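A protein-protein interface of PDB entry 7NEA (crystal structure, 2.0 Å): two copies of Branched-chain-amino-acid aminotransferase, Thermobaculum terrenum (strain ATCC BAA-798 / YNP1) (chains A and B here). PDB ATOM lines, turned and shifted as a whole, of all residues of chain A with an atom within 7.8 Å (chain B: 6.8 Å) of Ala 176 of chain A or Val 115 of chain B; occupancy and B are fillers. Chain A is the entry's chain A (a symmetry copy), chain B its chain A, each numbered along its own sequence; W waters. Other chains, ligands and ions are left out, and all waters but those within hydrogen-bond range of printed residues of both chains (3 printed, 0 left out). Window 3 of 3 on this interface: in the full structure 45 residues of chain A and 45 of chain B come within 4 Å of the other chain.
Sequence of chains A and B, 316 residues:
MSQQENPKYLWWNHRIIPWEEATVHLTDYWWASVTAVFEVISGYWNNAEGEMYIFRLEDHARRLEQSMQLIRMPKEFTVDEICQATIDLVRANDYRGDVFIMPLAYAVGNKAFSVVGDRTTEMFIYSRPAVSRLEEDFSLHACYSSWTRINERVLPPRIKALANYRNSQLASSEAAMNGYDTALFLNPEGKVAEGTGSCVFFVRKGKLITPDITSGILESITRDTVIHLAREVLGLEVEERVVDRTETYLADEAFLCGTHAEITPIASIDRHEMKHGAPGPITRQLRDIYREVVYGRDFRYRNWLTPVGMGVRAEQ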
ATOM      1  N   CYS A 143      -9.751 -20.004   3.431  1.00  0.00           N
ATOM      2  CA  CYS A 143     -10.700 -20.317   4.497  1.00  0.00           C
ATOM      3  C   CYS A 143     -10.704 -21.816   4.723  1.00  0.00           C
ATOM      4  O   CYS A 143     -10.448 -22.585   3.773  1.00  0.00           O
ATOM      5  CB  CYS A 143     -12.109 -19.814   4.206  1.00  0.00           C
ATOM      6  SG  CYS A 143     -12.838 -20.397   2.645  1.00  0.00           S
ATOM      7  N   GLN A 169     -15.185 -29.188  -5.170  1.00  0.00           N
ATOM      8  CA  GLN A 169     -15.925 -27.999  -5.727  1.00  0.00           C
ATOM      9  C   GLN A 169     -16.889 -27.430  -4.679  1.00  0.00           C
ATOM     10  O   GLN A 169     -17.150 -26.217  -4.702  1.00  0.00           O
ATOM     11  CB  GLN A 169     -16.686 -28.419  -6.953  1.00  0.00           C
ATOM     12  CG  GLN A 169     -15.757 -28.569  -8.139  1.00  0.00           C
ATOM     13  CD  GLN A 169     -16.460 -29.135  -9.352  1.00  0.00           C
ATOM     14  OE1 GLN A 169     -17.657 -29.564  -9.345  1.00  0.00           O
ATOM     15  NE2 GLN A 169     -15.699 -29.105 -10.442  1.00  0.00           N
ATOM     16  N   LEU A 170     -17.399 -28.270  -3.764  1.00  0.00           N
ATOM     17  CA  LEU A 170     -18.246 -27.725  -2.660  1.00  0.00           C
ATOM     18  C   LEU A 170     -17.433 -26.638  -1.913  1.00  0.00           C
ATOM     19  O   LEU A 170     -17.950 -25.543  -1.629  1.00  0.00           O
ATOM     20  CB  LEU A 170     -18.659 -28.845  -1.687  1.00  0.00           C
ATOM     21  CG  LEU A 170     -19.654 -29.851  -2.232  1.00  0.00           C
ATOM     22  CD1 LEU A 170     -19.723 -31.087  -1.307  1.00  0.00           C
ATOM     23  CD2 LEU A 170     -21.048 -29.209  -2.416  1.00  0.00           C
ATOM     24  N   ALA A 171     -16.191 -26.957  -1.566  1.00  0.00           N
ATOM     25  CA  ALA A 171     -15.297 -26.069  -0.821  1.00  0.00           C
ATOM     26  C   ALA A 171     -14.844 -24.881  -1.694  1.00  0.00           C
ATOM     27  O   ALA A 171     -14.838 -23.726  -1.198  1.00  0.00           O
ATOM     28  CB  ALA A 171     -14.159 -26.881  -0.255  1.00  0.00           C
ATOM     29  N   SER A 172     -14.393 -25.107  -2.910  1.00  0.00           N
ATOM     30  CA  SER A 172     -13.820 -24.017  -3.745  1.00  0.00           C
ATOM     31  C   SER A 172     -14.910 -23.043  -4.154  1.00  0.00           C
ATOM     32  O   SER A 172     -14.626 -21.831  -4.224  1.00  0.00           O
ATOM     33  CB  SER A 172     -13.001 -24.574  -4.931  1.00  0.00           C
ATOM     34  OG  SER A 172     -13.858 -25.377  -5.656  1.00  0.00           O
ATOM     35  N   SER A 173     -16.132 -23.516  -4.389  1.00  0.00           N
ATOM     36  CA  SER A 173     -17.308 -22.617  -4.602  1.00  0.00           C
ATOM     37  C   SER A 173     -17.522 -21.738  -3.375  1.00  0.00           C
ATOM     38  O   SER A 173     -17.711 -20.540  -3.497  1.00  0.00           O
ATOM     39  CB  SER A 173     -18.589 -23.412  -4.890  1.00  0.00           C
ATOM     40  OG  SER A 173     -18.554 -23.924  -6.205  1.00  0.00           O
ATOM     41  N   GLU A 174     -17.581 -22.346  -2.202  1.00  0.00           N
ATOM     42  CA  GLU A 174     -17.841 -21.582  -0.978  1.00  0.00           C
ATOM     43  C   GLU A 174     -16.743 -20.530  -0.814  1.00  0.00           C
ATOM     44  O   GLU A 174     -17.026 -19.359  -0.495  1.00  0.00           O
ATOM     45  CB  GLU A 174     -17.832 -22.561   0.216  1.00  0.00           C
ATOM     46  CG  GLU A 174     -17.978 -21.837   1.534  1.00  0.00           C
ATOM     47  CD  GLU A 174     -18.111 -22.762   2.741  1.00  0.00           C
ATOM     48  OE1 GLU A 174     -17.218 -23.595   2.982  1.00  0.00           O
ATOM     49  OE2 GLU A 174     -19.072 -22.580   3.486  1.00  0.00           O
ATOM     50  N   ALA A 175     -15.476 -20.925  -1.018  1.00  0.00           N
ATOM     51  CA  ALA A 175     -14.358 -19.987  -0.776  1.00  0.00           C
ATOM     52  C   ALA A 175     -14.521 -18.747  -1.669  1.00  0.00           C
ATOM     53  O   ALA A 175     -14.419 -17.572  -1.179  1.00  0.00           O
ATOM     54  CB  ALA A 175     -13.061 -20.684  -0.977  1.00  0.00           C
ATOM     55  N   ALA A 176     -14.766 -18.959  -2.944  1.00  0.00           N
ATOM     56  CA  ALA A 176     -14.836 -17.850  -3.923  1.00  0.00           C
ATOM     57  C   ALA A 176     -16.037 -16.963  -3.608  1.00  0.00           C
ATOM     58  O   ALA A 176     -15.909 -15.745  -3.601  1.00  0.00           O
ATOM     59  CB  ALA A 176     -14.907 -18.428  -5.344  1.00  0.00           C
ATOM     60  N   MET A 177     -17.207 -17.504  -3.290  1.00  0.00           N
ATOM     61  CA  MET A 177     -18.353 -16.583  -3.051  1.00  0.00           C
ATOM     62  C   MET A 177     -18.186 -15.923  -1.664  1.00  0.00           C
ATOM     63  O   MET A 177     -18.867 -14.946  -1.426  1.00  0.00           O
ATOM     64  CB  MET A 177     -19.724 -17.279  -3.137  1.00  0.00           C
ATOM     65  CG  MET A 177     -20.061 -18.190  -1.890  1.00  0.00           C
ATOM     66  SD  MET A 177     -21.646 -19.114  -2.165  1.00  0.00           S
ATOM     67  CE  MET A 177     -21.036 -20.360  -3.301  1.00  0.00           C
ATOM     68  N   ASN A 178     -17.337 -16.451  -0.767  1.00  0.00           N
ATOM     69  CA  ASN A 178     -17.115 -15.814   0.549  1.00  0.00           C
ATOM     70  C   ASN A 178     -15.860 -14.910   0.586  1.00  0.00           C
ATOM     71  O   ASN A 178     -15.519 -14.491   1.705  1.00  0.00           O
ATOM     72  CB  ASN A 178     -17.131 -16.860   1.649  1.00  0.00           C
ATOM     73  CG  ASN A 178     -18.502 -17.469   1.812  1.00  0.00           C
ATOM     74  OD1 ASN A 178     -19.500 -16.949   1.300  1.00  0.00           O
ATOM     75  ND2 ASN A 178     -18.574 -18.483   2.658  1.00  0.00           N
ATOM     76  N   GLY A 179     -15.227 -14.576  -0.531  1.00  0.00           N
ATOM     77  CA  GLY A 179     -14.178 -13.521  -0.612  1.00  0.00           C
ATOM     78  C   GLY A 179     -12.766 -14.089  -0.441  1.00  0.00           C
ATOM     79  O   GLY A 179     -11.851 -13.348  -0.103  1.00  0.00           O
ATOM     80  N   TYR A 180     -12.578 -15.408  -0.549  1.00  0.00           N
ATOM     81  CA  TYR A 180     -11.289 -16.055  -0.342  1.00  0.00           C
ATOM     82  C   TYR A 180     -10.773 -16.518  -1.695  1.00  0.00           C
ATOM     83  O   TYR A 180     -11.610 -16.621  -2.598  1.00  0.00           O
ATOM     84  CB  TYR A 180     -11.424 -17.209   0.632  1.00  0.00           C
ATOM     85  CG  TYR A 180     -11.771 -16.823   2.041  1.00  0.00           C
ATOM     86  CD1 TYR A 180     -10.826 -16.320   2.920  1.00  0.00           C
ATOM     87  CD2 TYR A 180     -13.087 -16.885   2.470  1.00  0.00           C
ATOM     88  CE1 TYR A 180     -11.186 -15.936   4.223  1.00  0.00           C
ATOM     89  CE2 TYR A 180     -13.469 -16.467   3.746  1.00  0.00           C
ATOM     90  CZ  TYR A 180     -12.501 -15.995   4.633  1.00  0.00           C
ATOM     91  OH  TYR A 180     -12.903 -15.715   5.919  1.00  0.00           O
ATOM     92  N   ASP A 181      -9.473 -16.813  -1.769  1.00  0.00           N
ATOM     93  CA  ASP A 181      -8.811 -17.331  -2.978  1.00  0.00           C
ATOM     94  C   ASP A 181      -8.874 -18.848  -2.990  1.00  0.00           C
ATOM     95  O   ASP A 181      -8.712 -19.413  -4.066  1.00  0.00           O
ATOM     96  CB  ASP A 181      -7.344 -16.906  -3.028  1.00  0.00           C
ATOM     97  CG  ASP A 181      -7.137 -15.406  -3.017  1.00  0.00           C
ATOM     98  OD1 ASP A 181      -7.872 -14.790  -3.731  1.00  0.00           O
ATOM     99  OD2 ASP A 181      -6.392 -14.875  -2.114  1.00  0.00           O
ATOM    100  N   THR A 182      -9.026 -19.531  -1.841  1.00  0.00           N
ATOM    101  CA  THR A 182      -8.809 -21.017  -1.843  1.00  0.00           C
ATOM    102  C   THR A 182      -9.382 -21.598  -0.561  1.00  0.00           C
ATOM    103  O   THR A 182      -9.463 -20.840   0.482  1.00  0.00           O
ATOM    104  CB  THR A 182      -7.323 -21.349  -2.061  1.00  0.00           C
ATOM    105  OG1 THR A 182      -7.170 -22.719  -2.412  1.00  0.00           O
ATOM    106  CG2 THR A 182      -6.464 -21.151  -0.831  1.00  0.00           C
ATOM    107  N   ALA A 183      -9.778 -22.882  -0.602  1.00  0.00           N
ATOM    108  CA  ALA A 183     -10.325 -23.522   0.604  1.00  0.00           C
ATOM    109  C   ALA A 183      -9.378 -24.585   1.156  1.00  0.00           C
ATOM    110  O   ALA A 183      -8.817 -25.370   0.360  1.00  0.00           O
ATOM    111  CB  ALA A 183     -11.684 -24.065   0.288  1.00  0.00           C
ATOM    112  N   GLY B 109     -15.686 -24.787 -17.970  1.00  0.00           N
ATOM    113  CA  GLY B 109     -14.797 -23.702 -17.496  1.00  0.00           C
ATOM    114  C   GLY B 109     -13.691 -23.367 -18.486  1.00  0.00           C
ATOM    115  O   GLY B 109     -13.418 -24.207 -19.369  1.00  0.00           O
ATOM    116  N   LYS B 111     -10.620 -22.794 -17.324  1.00  0.00           N
ATOM    117  CA  LYS B 111      -9.513 -23.504 -16.616  1.00  0.00           C
ATOM    118  C   LYS B 111     -10.095 -24.750 -15.924  1.00  0.00           C
ATOM    119  O   LYS B 111     -11.305 -24.709 -15.592  1.00  0.00           O
ATOM    120  CB  LYS B 111      -8.841 -22.561 -15.602  1.00  0.00           C
ATOM    121  N   PHE B 113      -9.902 -25.991 -12.893  1.00  0.00           N
ATOM    122  CA  PHE B 113     -10.332 -25.788 -11.471  1.00  0.00           C
ATOM    123  C   PHE B 113     -10.982 -24.399 -11.215  1.00  0.00           C
ATOM    124  O   PHE B 113     -11.082 -23.979 -10.022  1.00  0.00           O
ATOM    125  CB  PHE B 113      -9.142 -26.037 -10.523  1.00  0.00           C
ATOM    126  CG  PHE B 113      -8.469 -27.385 -10.676  1.00  0.00           C
ATOM    127  CD1 PHE B 113      -9.039 -28.541 -10.146  1.00  0.00           C
ATOM    128  CD2 PHE B 113      -7.274 -27.512 -11.372  1.00  0.00           C
ATOM    129  CE1 PHE B 113      -8.428 -29.777 -10.312  1.00  0.00           C
ATOM    130  CE2 PHE B 113      -6.662 -28.748 -11.520  1.00  0.00           C
ATOM    131  CZ  PHE B 113      -7.233 -29.877 -10.986  1.00  0.00           C
ATOM    132  N   SER B 114     -11.479 -23.715 -12.258  1.00  0.00           N
ATOM    133  CA  SER B 114     -12.351 -22.511 -12.133  1.00  0.00           C
ATOM    134  C   SER B 114     -13.593 -22.864 -11.286  1.00  0.00           C
ATOM    135  O   SER B 114     -14.066 -24.040 -11.354  1.00  0.00           O
ATOM    136  CB  SER B 114     -12.765 -21.978 -13.496  1.00  0.00           C
ATOM    137  OG  SER B 114     -13.645 -22.881 -14.162  1.00  0.00           O
ATOM    138  N   VAL B 115     -14.156 -21.909 -10.536  1.00  0.00           N
ATOM    139  CA  VAL B 115     -15.345 -22.238  -9.689  1.00  0.00           C
ATOM    140  C   VAL B 115     -16.563 -22.355 -10.613  1.00  0.00           C
ATOM    141  O   VAL B 115     -16.629 -21.674 -11.701  1.00  0.00           O
ATOM    142  CB  VAL B 115     -15.499 -21.309  -8.461  1.00  0.00           C
ATOM    143  CG1 VAL B 115     -14.139 -21.227  -7.728  1.00  0.00           C
ATOM    144  CG2 VAL B 115     -16.039 -19.915  -8.788  1.00  0.00           C
ATOM    145  N   VAL B 116     -17.448 -23.280 -10.248  1.00  0.00           N
ATOM    146  CA  VAL B 116     -18.633 -23.680 -11.061  1.00  0.00           C
ATOM    147  C   VAL B 116     -19.394 -22.414 -11.506  1.00  0.00           C
ATOM    148  O   VAL B 116     -19.758 -22.339 -12.672  1.00  0.00           O
ATOM    149  CB  VAL B 116     -19.537 -24.675 -10.306  1.00  0.00           C
ATOM    150  CG1 VAL B 116     -20.850 -24.836 -11.082  1.00  0.00           C
ATOM    151  CG2 VAL B 116     -18.821 -26.018 -10.110  1.00  0.00           C
ATOM    152  N   GLY B 117     -19.622 -21.460 -10.575  1.00  0.00           N
ATOM    153  CA  GLY B 117     -20.389 -20.235 -10.852  1.00  0.00           C
ATOM    154  C   GLY B 117     -19.774 -19.343 -11.940  1.00  0.00           C
ATOM    155  O   GLY B 117     -20.531 -18.443 -12.387  1.00  0.00           O
ATOM    156  N   ASP B 118     -18.490 -19.523 -12.322  1.00  0.00           N
ATOM    157  CA  ASP B 118     -17.785 -18.751 -13.420  1.00  0.00           C
ATOM    158  C   ASP B 118     -17.828 -19.529 -14.760  1.00  0.00           C
ATOM    159  O   ASP B 118     -17.280 -19.075 -15.801  1.00  0.00           O
ATOM    160  CB  ASP B 118     -16.331 -18.443 -13.039  1.00  0.00           C
ATOM    161  CG  ASP B 118     -16.196 -17.475 -11.857  1.00  0.00           C
ATOM    162  OD1 ASP B 118     -17.198 -16.800 -11.519  1.00  0.00           O
ATOM    163  OD2 ASP B 118     -15.096 -17.444 -11.238  1.00  0.00           O
ATOM    164  N   ARG B 119     -18.422 -20.717 -14.745  1.00  0.00           N
ATOM    165  CA  ARG B 119     -18.457 -21.604 -15.928  1.00  0.00           C
ATOM    166  C   ARG B 119     -19.650 -21.238 -16.829  1.00  0.00           C
ATOM    167  O   ARG B 119     -20.381 -20.282 -16.554  1.00  0.00           O
ATOM    168  CB  ARG B 119     -18.311 -23.031 -15.392  1.00  0.00           C
ATOM    169  CG  ARG B 119     -16.864 -23.271 -14.962  1.00  0.00           C
ATOM    170  CD  ARG B 119     -16.494 -24.123 -13.773  1.00  0.00           C
ATOM    171  NE  ARG B 119     -16.472 -25.488 -14.183  1.00  0.00           N
ATOM    172  CZ  ARG B 119     -15.727 -26.469 -13.681  1.00  0.00           C
ATOM    173  NH1 ARG B 119     -14.832 -26.244 -12.739  1.00  0.00           N
ATOM    174  NH2 ARG B 119     -15.862 -27.685 -14.191  1.00  0.00           N
HETATM  175  O   HOH W   1     -14.413 -29.619 -12.847  1.00  0.00           O
HETATM  176  O   HOH W   2     -19.793 -21.513  -7.449  1.00  0.00           O
HETATM  177  O   HOH W   3     -16.442 -24.836  -7.587  1.00  0.00           O
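Water W3 lies within hydrogen-bond range of the side-chain hydroxyl of Ser 173 of chain A (2.7 Å), the backbone NH of Val 116 of chain B (3.2 Å), the side-chain hydroxyl of Ser 172 of chain A (3.3 Å) and the backbone carbonyl oxygen of Gln 169 of chain A (3.3 Å).
Water W1 lies within hydrogen-bond range of NH2 of Arg 119 of chain B (2.8 Å) and NE2 of Gln 169 of chain A (2.8 Å).
Water W2 lies within hydrogen-bond range of OG of Ser 173 of chain A (3.0 Å) and N of Gly 117 of chain B (3.1 Å).
Of the printed residues of chain B, Gln 169 of chain A touches Val 116 (3.8 Å) and Arg 119 (3.8 Å).
Ala 171 of chain A touches none of the printed residues of chain B.
Printed residues of chain B within 4 Å of Ser 172 of chain A: Val 115 (3.6 Å).
Of chain B, only Val 115 (3.8 Å) comes within 4 Å of Ala 176 of chain A.
Lys 111 of chain B touches none of the printed residues of chain A.
Val 115 of chain B touches just these residues of chain A: Ser 172 (3.6 Å) and Ala 176 (3.8 Å).
Of the printed residues of chain A, Val 116 of chain B touches Gln 169 (3.8 Å).
Of the printed residues of chain A, Arg 119 of chain B touches Gln 169 (3.8 Å).
The nearest residue of chain B that does not touch Ala 176 of chain A is Asp 118 of chain B (6.0 Å).
The nearest printed residue of chain B that does not touch Ser 172 of chain A is Phe 113 of chain B (5.4 Å).
NH1 of Arg 119 of chain B lies within hydrogen-bond range of O of Ser 114 of chain B (2.7 Å).
O of Gln 169 of chain A lies within hydrogen-bond range of OG of Ser 173 of chain A (3.1 Å).
OE1 of Gln 169 of chain A touches CG2 of Val 116 of chain B, at 3.8 Å.
NE2 of Gln 169 of chain A touches NH1 of Arg 119 of chain B, 3.8 Å away.
Val 115 of chain B touches Ser 172 of chain A.
CG1 of Val 115 of chain B touches CB of Ala 176 of chain A (3.8 Å).
No position is printed for both chains.
Of the 16 printed residues of chain A, 3 touch a printed residue of chain B.
Hydrophobic or aromatic side chains of chain A that line the printed part of chain B: Ala 176.
Of the 9 printed residues of chain B, 3 touch a printed residue of chain A.
Hydrophobic or aromatic side chains of chain B within 4 Å of the printed part of chain A: Val 115 and Val 116.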
